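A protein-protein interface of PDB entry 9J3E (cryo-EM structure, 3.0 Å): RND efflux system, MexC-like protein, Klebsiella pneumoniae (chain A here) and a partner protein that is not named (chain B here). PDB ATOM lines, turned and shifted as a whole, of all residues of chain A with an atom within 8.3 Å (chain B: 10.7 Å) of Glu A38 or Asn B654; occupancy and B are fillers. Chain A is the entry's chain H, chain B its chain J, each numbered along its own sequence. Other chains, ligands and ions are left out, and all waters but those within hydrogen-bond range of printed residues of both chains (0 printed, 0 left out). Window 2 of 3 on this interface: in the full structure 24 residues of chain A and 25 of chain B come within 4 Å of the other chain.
NE of Arg A37 sits at hydrogen-bond distance from O of Ala B653 (3.0 Å).
The guanidinium group (NH1) of Arg A37 lies within hydrogen-bond range of the backbone carbonyl oxygen (O) of Leu B655 (2.7 Å).
The backbone NH (N) of Glu A38 is in hydrogen-bond range of the side-chain amide oxygen (OD1) of Asn B654.
The backbone NH (N) of Ser A360 is in hydrogen-bond range of the backbone carbonyl oxygen (O) of Asp B656 (2.6 Å).
The guanidinium group (NH1) of Arg A373 sits close to the side-chain amide nitrogen (ND2) of Asn B654 (2.9 Å).
The guanidinium group (NH1) of Arg A37 is in hydrogen-bond range of the side-chain hydroxyl (OG) of Ser A360, at 3.3 Å.
N of Ile A371 lies within hydrogen-bond range of O of Arg A37, 3.3 Å away.
OE1 of Glu A38 lies within salt-bridge range of NH1 of Arg A373, 3.9 Å away.
The backbone carbonyl oxygen of Val A39 lies within hydrogen-bond range of the backbone NH of Arg A373 (3.0 Å).
The backbone NH of Asp A40 is in hydrogen-bond range of the side-chain hydroxyl of Ser A359 (2.5 Å).
The guanidinium group (NE) of Arg A373 is in salt-bridge range of the side-chain carboxylate (OD1) of Asp A40.
Among the printed residues, merely in contact across the chains: Arg A37 with Asn B654 (3.3 Å), Asp A40 with Asp B656 (3.8 Å), Ser A359 with Asp B656 (3.5 Å), Ser A360 with Leu B655 (3.6 Å) and Arg A373 with Asp B656 (3.9 Å).
No residue of chain B comes within 4 Å of Ala A36.
Printed residues of chain B within 4 Å of Arg A37: Ala B653 (2.3 Å), Asn B654 (3.3 Å) and Leu B655 (2.7 Å).
No residue of chain B comes within 4 Å of Val A39.
Val A41 touches none of the printed residues of chain B.
Printed residues of chain B within 4 Å of Ser A360: Leu B655 and Asp B656.
Val A370 touches none of the printed residues of chain B.
No residue of chain B comes within 4 Å of Ile A371.
Printed residues of chain B within 4 Å of Arg A373: Asn B654 (2.9 Å) and Asp B656 (3.9 Å).
Of chain A, only Arg A37 (2.3 Å) comes within 4 Å of Ala B653.
Of the printed residues of chain A, Asn B654 touches Arg A37 (3.3 Å), Glu A38 (2.9 Å) and Arg A373 (2.9 Å).
Of the printed residues of chain A, Leu B655 touches Arg A37 and Ser A360.
The nearest residue of chain B that does not touch Glu A38 is Asp B656 (5.5 Å).
The nearest residue of chain A that does not touch Asn B654 is Ala A36 (4.5 Å).
Of the 17 printed residues of chain B, 4 touch a printed residue of chain A.
Of the 16 printed residues of chain A, 6 touch a printed residue of chain B.
Printed residues of chain A that touch a printed residue of chain B: Arg A37, Glu A38, Asp A40, Ser A359, Ser A360 and Arg A373.
Along chain A the printed residues that touch a printed residue of chain B span positions 37 to 373.
Among the printed residues, 10 pairs touch across the chains.
Among the printed residues, no Asp or Glu carboxylate lies within 4 Å of a Lys or Arg side-chain nitrogen of the other chain.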
ATOM      1  N   ALA A  36      32.839  -3.006  -0.129  1.00  0.00           N
ATOM      2  CA  ALA A  36      31.428  -3.361  -0.212  1.00  0.00           C
ATOM      3  C   ALA A  36      30.906  -3.128  -1.619  1.00  0.00           C
ATOM      4  O   ALA A  36      31.099  -2.057  -2.188  1.00  0.00           O
ATOM      5  CB  ALA A  36      30.622  -2.564   0.790  1.00  0.00           C
ATOM      6  N   ARG A  37      30.247  -4.133  -2.183  1.00  0.00           N
ATOM      7  CA  ARG A  37      29.779  -4.035  -3.556  1.00  0.00           C
ATOM      8  C   ARG A  37      28.439  -3.320  -3.622  1.00  0.00           C
ATOM      9  O   ARG A  37      27.466  -3.735  -2.989  1.00  0.00           O
ATOM     10  CB  ARG A  37      29.657  -5.421  -4.182  1.00  0.00           C
ATOM     11  CG  ARG A  37      29.750  -5.376  -5.689  1.00  0.00           C
ATOM     12  CD  ARG A  37      29.823  -6.748  -6.316  1.00  0.00           C
ATOM     13  NE  ARG A  37      30.837  -6.783  -7.363  1.00  0.00           N
ATOM     14  CZ  ARG A  37      30.716  -7.439  -8.507  1.00  0.00           C
ATOM     15  NH1 ARG A  37      29.608  -8.093  -8.814  1.00  0.00           N
ATOM     16  NH2 ARG A  37      31.724  -7.427  -9.372  1.00  0.00           N
ATOM     17  N   GLU A  38      28.388  -2.250  -4.410  1.00  0.00           N
ATOM     18  CA  GLU A  38      27.148  -1.514  -4.594  1.00  0.00           C
ATOM     19  C   GLU A  38      26.175  -2.347  -5.411  1.00  0.00           C
ATOM     20  O   GLU A  38      26.524  -2.855  -6.480  1.00  0.00           O
ATOM     21  CB  GLU A  38      27.407  -0.178  -5.285  1.00  0.00           C
ATOM     22  CG  GLU A  38      28.014   0.870  -4.380  1.00  0.00           C
ATOM     23  CD  GLU A  38      27.948   2.258  -4.979  1.00  0.00           C
ATOM     24  OE1 GLU A  38      27.326   2.415  -6.050  1.00  0.00           O
ATOM     25  OE2 GLU A  38      28.512   3.194  -4.374  1.00  0.00           O
ATOM     26  N   VAL A  39      24.950  -2.476  -4.914  1.00  0.00           N
ATOM     27  CA  VAL A  39      23.962  -3.362  -5.506  1.00  0.00           C
ATOM     28  C   VAL A  39      22.667  -2.600  -5.725  1.00  0.00           C
ATOM     29  O   VAL A  39      22.343  -1.662  -4.990  1.00  0.00           O
ATOM     30  CB  VAL A  39      23.710  -4.595  -4.621  1.00  0.00           C
ATOM     31  CG1 VAL A  39      24.985  -5.379  -4.454  1.00  0.00           C
ATOM     32  CG2 VAL A  39      23.185  -4.166  -3.276  1.00  0.00           C
ATOM     33  N   ASP A  40      21.925  -3.005  -6.750  1.00  0.00           N
ATOM     34  CA  ASP A  40      20.596  -2.457  -6.969  1.00  0.00           C
ATOM     35  C   ASP A  40      19.613  -3.155  -6.042  1.00  0.00           C
ATOM     36  O   ASP A  40      19.580  -4.387  -5.971  1.00  0.00           O
ATOM     37  CB  ASP A  40      20.166  -2.624  -8.424  1.00  0.00           C
ATOM     38  CG  ASP A  40      20.898  -1.687  -9.356  1.00  0.00           C
ATOM     39  OD1 ASP A  40      21.421  -0.661  -8.877  1.00  0.00           O
ATOM     40  OD2 ASP A  40      20.939  -1.963 -10.571  1.00  0.00           O
ATOM     41  N   VAL A  41      18.822  -2.367  -5.327  1.00  0.00           N
ATOM     42  CA  VAL A  41      17.882  -2.876  -4.341  1.00  0.00           C
ATOM     43  C   VAL A  41      16.477  -2.538  -4.805  1.00  0.00           C
ATOM     44  O   VAL A  41      16.197  -1.391  -5.164  1.00  0.00           O
ATOM     45  CB  VAL A  41      18.147  -2.286  -2.946  1.00  0.00           C
ATOM     46  CG1 VAL A  41      17.270  -2.960  -1.918  1.00  0.00           C
ATOM     47  CG2 VAL A  41      19.600  -2.448  -2.591  1.00  0.00           C
ATOM     48  N   ILE A 357      17.564  -7.645  -3.227  1.00  0.00           N
ATOM     49  CA  ILE A 357      18.719  -7.217  -4.005  1.00  0.00           C
ATOM     50  C   ILE A 357      18.620  -7.857  -5.378  1.00  0.00           C
ATOM     51  O   ILE A 357      18.474  -9.080  -5.492  1.00  0.00           O
ATOM     52  CB  ILE A 357      20.035  -7.598  -3.303  1.00  0.00           C
ATOM     53  CG1 ILE A 357      20.526  -6.460  -2.414  1.00  0.00           C
ATOM     54  CG2 ILE A 357      21.109  -7.922  -4.311  1.00  0.00           C
ATOM     55  CD1 ILE A 357      19.485  -5.885  -1.498  1.00  0.00           C
ATOM     56  N   SER A 359      20.957  -7.492  -8.000  1.00  0.00           N
ATOM     57  CA  SER A 359      22.215  -7.316  -8.705  1.00  0.00           C
ATOM     58  C   SER A 359      23.336  -7.976  -7.918  1.00  0.00           C
ATOM     59  O   SER A 359      23.213  -8.228  -6.718  1.00  0.00           O
ATOM     60  CB  SER A 359      22.511  -5.835  -8.929  1.00  0.00           C
ATOM     61  OG  SER A 359      22.751  -5.188  -7.698  1.00  0.00           O
ATOM     62  N   SER A 360      24.431  -8.270  -8.620  1.00  0.00           N
ATOM     63  CA  SER A 360      25.644  -8.822  -8.017  1.00  0.00           C
ATOM     64  C   SER A 360      25.371 -10.106  -7.246  1.00  0.00           C
ATOM     65  O   SER A 360      26.098 -10.444  -6.310  1.00  0.00           O
ATOM     66  CB  SER A 360      26.326  -7.800  -7.106  1.00  0.00           C
ATOM     67  OG  SER A 360      26.788  -6.687  -7.844  1.00  0.00           O
ATOM     68  N   ALA A 363      28.252 -12.237  -6.803  1.00  0.00           N
ATOM     69  CA  ALA A 363      29.347 -11.714  -6.000  1.00  0.00           C
ATOM     70  C   ALA A 363      28.930 -11.364  -4.581  1.00  0.00           C
ATOM     71  O   ALA A 363      29.596 -10.551  -3.935  1.00  0.00           O
ATOM     72  CB  ALA A 363      29.959 -10.490  -6.677  1.00  0.00           C
ATOM     73  N   ILE A 364      27.840 -11.938  -4.083  1.00  0.00           N
ATOM     74  CA  ILE A 364      27.362 -11.676  -2.734  1.00  0.00           C
ATOM     75  C   ILE A 364      27.234 -12.993  -1.987  1.00  0.00           C
ATOM     76  O   ILE A 364      26.611 -13.937  -2.485  1.00  0.00           O
ATOM     77  CB  ILE A 364      26.019 -10.929  -2.743  1.00  0.00           C
ATOM     78  CG1 ILE A 364      26.205  -9.503  -3.246  1.00  0.00           C
ATOM     79  CG2 ILE A 364      25.414 -10.920  -1.367  1.00  0.00           C
ATOM     80  CD1 ILE A 364      24.915  -8.855  -3.652  1.00  0.00           C
ATOM     81  N   LYS A 369      28.612  -7.405   3.842  1.00  0.00           N
ATOM     82  CA  LYS A 369      28.169  -6.019   3.867  1.00  0.00           C
ATOM     83  C   LYS A 369      28.139  -5.456   2.454  1.00  0.00           C
ATOM     84  O   LYS A 369      29.120  -5.569   1.714  1.00  0.00           O
ATOM     85  CB  LYS A 369      29.082  -5.178   4.755  1.00  0.00           C
ATOM     86  CG  LYS A 369      28.515  -4.913   6.132  1.00  0.00           C
ATOM     87  CD  LYS A 369      27.560  -3.738   6.086  1.00  0.00           C
ATOM     88  CE  LYS A 369      28.219  -2.526   5.456  1.00  0.00           C
ATOM     89  NZ  LYS A 369      27.218  -1.515   5.028  1.00  0.00           N
ATOM     90  N   VAL A 370      27.011  -4.855   2.081  1.00  0.00           N
ATOM     91  CA  VAL A 370      26.806  -4.339   0.737  1.00  0.00           C
ATOM     92  C   VAL A 370      26.266  -2.920   0.820  1.00  0.00           C
ATOM     93  O   VAL A 370      25.751  -2.482   1.849  1.00  0.00           O
ATOM     94  CB  VAL A 370      25.848  -5.220  -0.081  1.00  0.00           C
ATOM     95  CG1 VAL A 370      26.238  -6.679   0.037  1.00  0.00           C
ATOM     96  CG2 VAL A 370      24.437  -5.014   0.391  1.00  0.00           C
ATOM     97  N   ILE A 371      26.389  -2.203  -0.290  1.00  0.00           N
ATOM     98  CA  ILE A 371      25.994  -0.804  -0.385  1.00  0.00           C
ATOM     99  C   ILE A 371      24.777  -0.716  -1.303  1.00  0.00           C
ATOM    100  O   ILE A 371      24.900  -0.921  -2.519  1.00  0.00           O
ATOM    101  CB  ILE A 371      27.140   0.072  -0.902  1.00  0.00           C
ATOM    102  CG1 ILE A 371      28.298   0.056   0.092  1.00  0.00           C
ATOM    103  CG2 ILE A 371      26.659   1.487  -1.120  1.00  0.00           C
ATOM    104  CD1 ILE A 371      29.532   0.757  -0.407  1.00  0.00           C
ATOM    105  N   PRO A 372      23.596  -0.403  -0.782  1.00  0.00           N
ATOM    106  CA  PRO A 372      22.426  -0.244  -1.649  1.00  0.00           C
ATOM    107  C   PRO A 372      22.579   0.963  -2.552  1.00  0.00           C
ATOM    108  O   PRO A 372      23.328   1.895  -2.252  1.00  0.00           O
ATOM    109  CB  PRO A 372      21.277  -0.052  -0.657  1.00  0.00           C
ATOM    110  CG  PRO A 372      21.927   0.517   0.548  1.00  0.00           C
ATOM    111  CD  PRO A 372      23.287  -0.105   0.625  1.00  0.00           C
ATOM    112  N   ARG A 373      21.873   0.938  -3.673  1.00  0.00           N
ATOM    113  CA  ARG A 373      21.876   2.075  -4.578  1.00  0.00           C
ATOM    114  C   ARG A 373      20.484   2.682  -4.683  1.00  0.00           C
ATOM    115  O   ARG A 373      20.186   3.684  -4.036  1.00  0.00           O
ATOM    116  CB  ARG A 373      22.374   1.658  -5.957  1.00  0.00           C
ATOM    117  CG  ARG A 373      23.881   1.618  -6.076  1.00  0.00           C
ATOM    118  CD  ARG A 373      24.299   1.319  -7.503  1.00  0.00           C
ATOM    119  NE  ARG A 373      24.151  -0.096  -7.824  1.00  0.00           N
ATOM    120  CZ  ARG A 373      25.109  -0.847  -8.345  1.00  0.00           C
ATOM    121  NH1 ARG A 373      26.302  -0.349  -8.625  1.00  0.00           N
ATOM    122  NH2 ARG A 373      24.865  -2.130  -8.594  1.00  0.00           N
ATOM    123  N   GLU B 593      27.984  -3.294 -22.601  1.00  0.00           N
ATOM    124  CA  GLU B 593      28.649  -2.375 -21.683  1.00  0.00           C
ATOM    125  C   GLU B 593      30.166  -2.548 -21.734  1.00  0.00           C
ATOM    126  O   GLU B 593      30.915  -1.560 -21.740  1.00  0.00           O
ATOM    127  CB  GLU B 593      28.123  -2.566 -20.266  1.00  0.00           C
ATOM    128  CG  GLU B 593      28.529  -1.450 -19.327  1.00  0.00           C
ATOM    129  CD  GLU B 593      27.902  -1.578 -17.956  1.00  0.00           C
ATOM    130  OE1 GLU B 593      27.032  -2.457 -17.778  1.00  0.00           O
ATOM    131  OE2 GLU B 593      28.278  -0.800 -17.056  1.00  0.00           O
ATOM    132  N   ALA B 646      44.283  -4.393 -15.788  1.00  0.00           N
ATOM    133  CA  ALA B 646      44.010  -4.003 -14.415  1.00  0.00           C
ATOM    134  C   ALA B 646      42.997  -2.873 -14.376  1.00  0.00           C
ATOM    135  O   ALA B 646      42.121  -2.843 -13.508  1.00  0.00           O
ATOM    136  CB  ALA B 646      45.303  -3.595 -13.715  1.00  0.00           C
ATOM    137  N   ALA B 647      43.102  -1.937 -15.317  1.00  0.00           N
ATOM    138  CA  ALA B 647      42.124  -0.858 -15.394  1.00  0.00           C
ATOM    139  C   ALA B 647      40.730  -1.400 -15.669  1.00  0.00           C
ATOM    140  O   ALA B 647      39.746  -0.932 -15.087  1.00  0.00           O
ATOM    141  CB  ALA B 647      42.534   0.142 -16.472  1.00  0.00           C
ATOM    142  N   VAL B 648      40.628  -2.388 -16.558  1.00  0.00           N
ATOM    143  CA  VAL B 648      39.329  -2.984 -16.856  1.00  0.00           C
ATOM    144  C   VAL B 648      38.772  -3.704 -15.634  1.00  0.00           C
ATOM    145  O   VAL B 648      37.614  -3.499 -15.254  1.00  0.00           O
ATOM    146  CB  VAL B 648      39.431  -3.929 -18.063  1.00  0.00           C
ATOM    147  CG1 VAL B 648      38.181  -4.770 -18.169  1.00  0.00           C
ATOM    148  CG2 VAL B 648      39.632  -3.132 -19.332  1.00  0.00           C
ATOM    149  N   ASN B 649      39.590  -4.539 -14.989  1.00  0.00           N
ATOM    150  CA  ASN B 649      39.125  -5.274 -13.816  1.00  0.00           C
ATOM    151  C   ASN B 649      38.699  -4.334 -12.702  1.00  0.00           C
ATOM    152  O   ASN B 649      37.693  -4.583 -12.032  1.00  0.00           O
ATOM    153  CB  ASN B 649      40.212  -6.217 -13.312  1.00  0.00           C
ATOM    154  CG  ASN B 649      40.450  -7.376 -14.242  1.00  0.00           C
ATOM    155  OD1 ASN B 649      39.630  -7.667 -15.106  1.00  0.00           O
ATOM    156  ND2 ASN B 649      41.574  -8.052 -14.067  1.00  0.00           N
ATOM    157  N   GLN B 650      39.441  -3.248 -12.495  1.00  0.00           N
ATOM    158  CA  GLN B 650      39.014  -2.234 -11.543  1.00  0.00           C
ATOM    159  C   GLN B 650      37.704  -1.598 -11.975  1.00  0.00           C
ATOM    160  O   GLN B 650      36.839  -1.318 -11.137  1.00  0.00           O
ATOM    161  CB  GLN B 650      40.094  -1.167 -11.398  1.00  0.00           C
ATOM    162  CG  GLN B 650      39.781  -0.117 -10.360  1.00  0.00           C
ATOM    163  CD  GLN B 650      40.822   0.978 -10.323  1.00  0.00           C
ATOM    164  OE1 GLN B 650      41.720   1.022 -11.165  1.00  0.00           O
ATOM    165  NE2 GLN B 650      40.707   1.874  -9.352  1.00  0.00           N
ATOM    166  N   HIS B 651      37.541  -1.348 -13.272  1.00  0.00           N
ATOM    167  CA  HIS B 651      36.337  -0.672 -13.734  1.00  0.00           C
ATOM    168  C   HIS B 651      35.119  -1.569 -13.601  1.00  0.00           C
ATOM    169  O   HIS B 651      34.077  -1.147 -13.089  1.00  0.00           O
ATOM    170  CB  HIS B 651      36.507  -0.214 -15.180  1.00  0.00           C
ATOM    171  CG  HIS B 651      35.231   0.234 -15.818  1.00  0.00           C
ATOM    172  ND1 HIS B 651      34.253  -0.644 -16.230  1.00  0.00           N
ATOM    173  CD2 HIS B 651      34.758   1.475 -16.085  1.00  0.00           C
ATOM    174  CE1 HIS B 651      33.241   0.035 -16.740  1.00  0.00           C
ATOM    175  NE2 HIS B 651      33.524   1.323 -16.666  1.00  0.00           N
ATOM    176  N   PHE B 652      35.225  -2.812 -14.059  1.00  0.00           N
ATOM    177  CA  PHE B 652      34.108  -3.736 -14.004  1.00  0.00           C
ATOM    178  C   PHE B 652      34.103  -4.564 -12.732  1.00  0.00           C
ATOM    179  O   PHE B 652      33.504  -5.643 -12.708  1.00  0.00           O
ATOM    180  CB  PHE B 652      34.117  -4.647 -15.227  1.00  0.00           C
ATOM    181  CG  PHE B 652      33.606  -3.988 -16.469  1.00  0.00           C
ATOM    182  CD1 PHE B 652      32.349  -3.426 -16.497  1.00  0.00           C
ATOM    183  CD2 PHE B 652      34.380  -3.933 -17.609  1.00  0.00           C
ATOM    184  CE1 PHE B 652      31.876  -2.823 -17.633  1.00  0.00           C
ATOM    185  CE2 PHE B 652      33.910  -3.330 -18.747  1.00  0.00           C
ATOM    186  CZ  PHE B 652      32.659  -2.773 -18.758  1.00  0.00           C
ATOM    187  N   ALA B 653      34.766  -4.091 -11.678  1.00  0.00           N
ATOM    188  CA  ALA B 653      34.745  -4.801 -10.408  1.00  0.00           C
ATOM    189  C   ALA B 653      33.384  -4.743  -9.741  1.00  0.00           C
ATOM    190  O   ALA B 653      33.056  -5.636  -8.955  1.00  0.00           O
ATOM    191  CB  ALA B 653      35.802  -4.233  -9.462  1.00  0.00           C
ATOM    192  N   ASN B 654      32.590  -3.720 -10.030  1.00  0.00           N
ATOM    193  CA  ASN B 654      31.277  -3.538  -9.430  1.00  0.00           C
ATOM    194  C   ASN B 654      30.180  -3.752 -10.464  1.00  0.00           C
ATOM    195  O   ASN B 654      29.114  -3.138 -10.406  1.00  0.00           O
ATOM    196  CB  ASN B 654      31.158  -2.158  -8.792  1.00  0.00           C
ATOM    197  CG  ASN B 654      30.017  -2.071  -7.809  1.00  0.00           C
ATOM    198  OD1 ASN B 654      30.208  -2.209  -6.603  1.00  0.00           O
ATOM    199  ND2 ASN B 654      28.815  -1.854  -8.322  1.00  0.00           N
ATOM    200  N   LEU B 655      30.437  -4.626 -11.432  1.00  0.00           N
ATOM    201  CA  LEU B 655      29.413  -4.977 -12.403  1.00  0.00           C
ATOM    202  C   LEU B 655      28.313  -5.776 -11.725  1.00  0.00           C
ATOM    203  O   LEU B 655      28.584  -6.670 -10.920  1.00  0.00           O
ATOM    204  CB  LEU B 655      30.008  -5.777 -13.554  1.00  0.00           C
ATOM    205  CG  LEU B 655      29.134  -5.852 -14.806  1.00  0.00           C
ATOM    206  CD1 LEU B 655      28.306  -4.589 -14.979  1.00  0.00           C
ATOM    207  CD2 LEU B 655      29.986  -6.102 -16.030  1.00  0.00           C
ATOM    208  N   ASP B 656      27.070  -5.458 -12.064  1.00  0.00           N
ATOM    209  CA  ASP B 656      25.916  -5.978 -11.351  1.00  0.00           C
ATOM    210  C   ASP B 656      25.365  -7.271 -11.930  1.00  0.00           C
ATOM    211  O   ASP B 656      24.672  -8.004 -11.217  1.00  0.00           O
ATOM    212  CB  ASP B 656      24.820  -4.915 -11.330  1.00  0.00           C
ATOM    213  CG  ASP B 656      24.444  -4.451 -12.715  1.00  0.00           C
ATOM    214  OD1 ASP B 656      25.165  -4.804 -13.671  1.00  0.00           O
ATOM    215  OD2 ASP B 656      23.438  -3.725 -12.849  1.00  0.00           O
ATOM    216  N   ASP B 657      25.649  -7.573 -13.192  1.00  0.00           N
ATOM    217  CA  ASP B 657      25.066  -8.721 -13.884  1.00  0.00           C
ATOM    218  C   ASP B 657      26.185  -9.629 -14.385  1.00  0.00           C
ATOM    219  O   ASP B 657      26.602  -9.534 -15.541  1.00  0.00           O
ATOM    220  CB  ASP B 657      24.180  -8.246 -15.030  1.00  0.00           C
ATOM    221  CG  ASP B 657      23.366  -9.362 -15.642  1.00  0.00           C
ATOM    222  OD1 ASP B 657      23.226 -10.420 -14.996  1.00  0.00           O
ATOM    223  OD2 ASP B 657      22.865  -9.178 -16.771  1.00  0.00           O
ATOM    224  N   GLY B 658      26.662 -10.516 -13.525  1.00  0.00           N
ATOM    225  CA  GLY B 658      27.680 -11.466 -13.910  1.00  0.00           C
ATOM    226  C   GLY B 658      29.062 -11.086 -13.425  1.00  0.00           C
ATOM    227  O   GLY B 658      29.244 -10.367 -12.439  1.00  0.00           O
ATOM    228  N   ALA B 659      30.059 -11.590 -14.145  1.00  0.00           N
ATOM    229  CA  ALA B 659      31.452 -11.370 -13.796  1.00  0.00           C
ATOM    230  C   ALA B 659      32.270 -11.116 -15.050  1.00  0.00           C
ATOM    231  O   ALA B 659      32.102 -11.803 -16.059  1.00  0.00           O
ATOM    232  CB  ALA B 659      32.031 -12.567 -13.039  1.00  0.00           C
ATOM    233  N   ILE B 660      33.160 -10.131 -14.975  1.00  0.00           N
ATOM    234  CA  ILE B 660      34.093  -9.810 -16.045  1.00  0.00           C
ATOM    235  C   ILE B 660      35.500  -9.947 -15.494  1.00  0.00           C
ATOM    236  O   ILE B 660      35.833  -9.334 -14.473  1.00  0.00           O
ATOM    237  CB  ILE B 660      33.872  -8.390 -16.590  1.00  0.00           C
ATOM    238  CG1 ILE B 660      32.581  -8.312 -17.400  1.00  0.00           C
ATOM    239  CG2 ILE B 660      35.043  -7.978 -17.439  1.00  0.00           C
ATOM    240  CD1 ILE B 660      32.308  -9.520 -18.209  1.00  0.00           C
ATOM    241  N   MET B 661      36.326 -10.737 -16.170  1.00  0.00           N
ATOM    242  CA  MET B 661      37.692 -10.988 -15.727  1.00  0.00           C
ATOM    243  C   MET B 661      38.619 -10.802 -16.913  1.00  0.00           C
ATOM    244  O   MET B 661      38.332 -11.298 -18.004  1.00  0.00           O
ATOM    245  CB  MET B 661      37.830 -12.398 -15.152  1.00  0.00           C
ATOM    246  CG  MET B 661      39.259 -12.865 -14.991  1.00  0.00           C
ATOM    247  SD  MET B 661      39.423 -14.220 -13.814  1.00  0.00           S
ATOM    248  CE  MET B 661      37.721 -14.754 -13.654  1.00  0.00           C
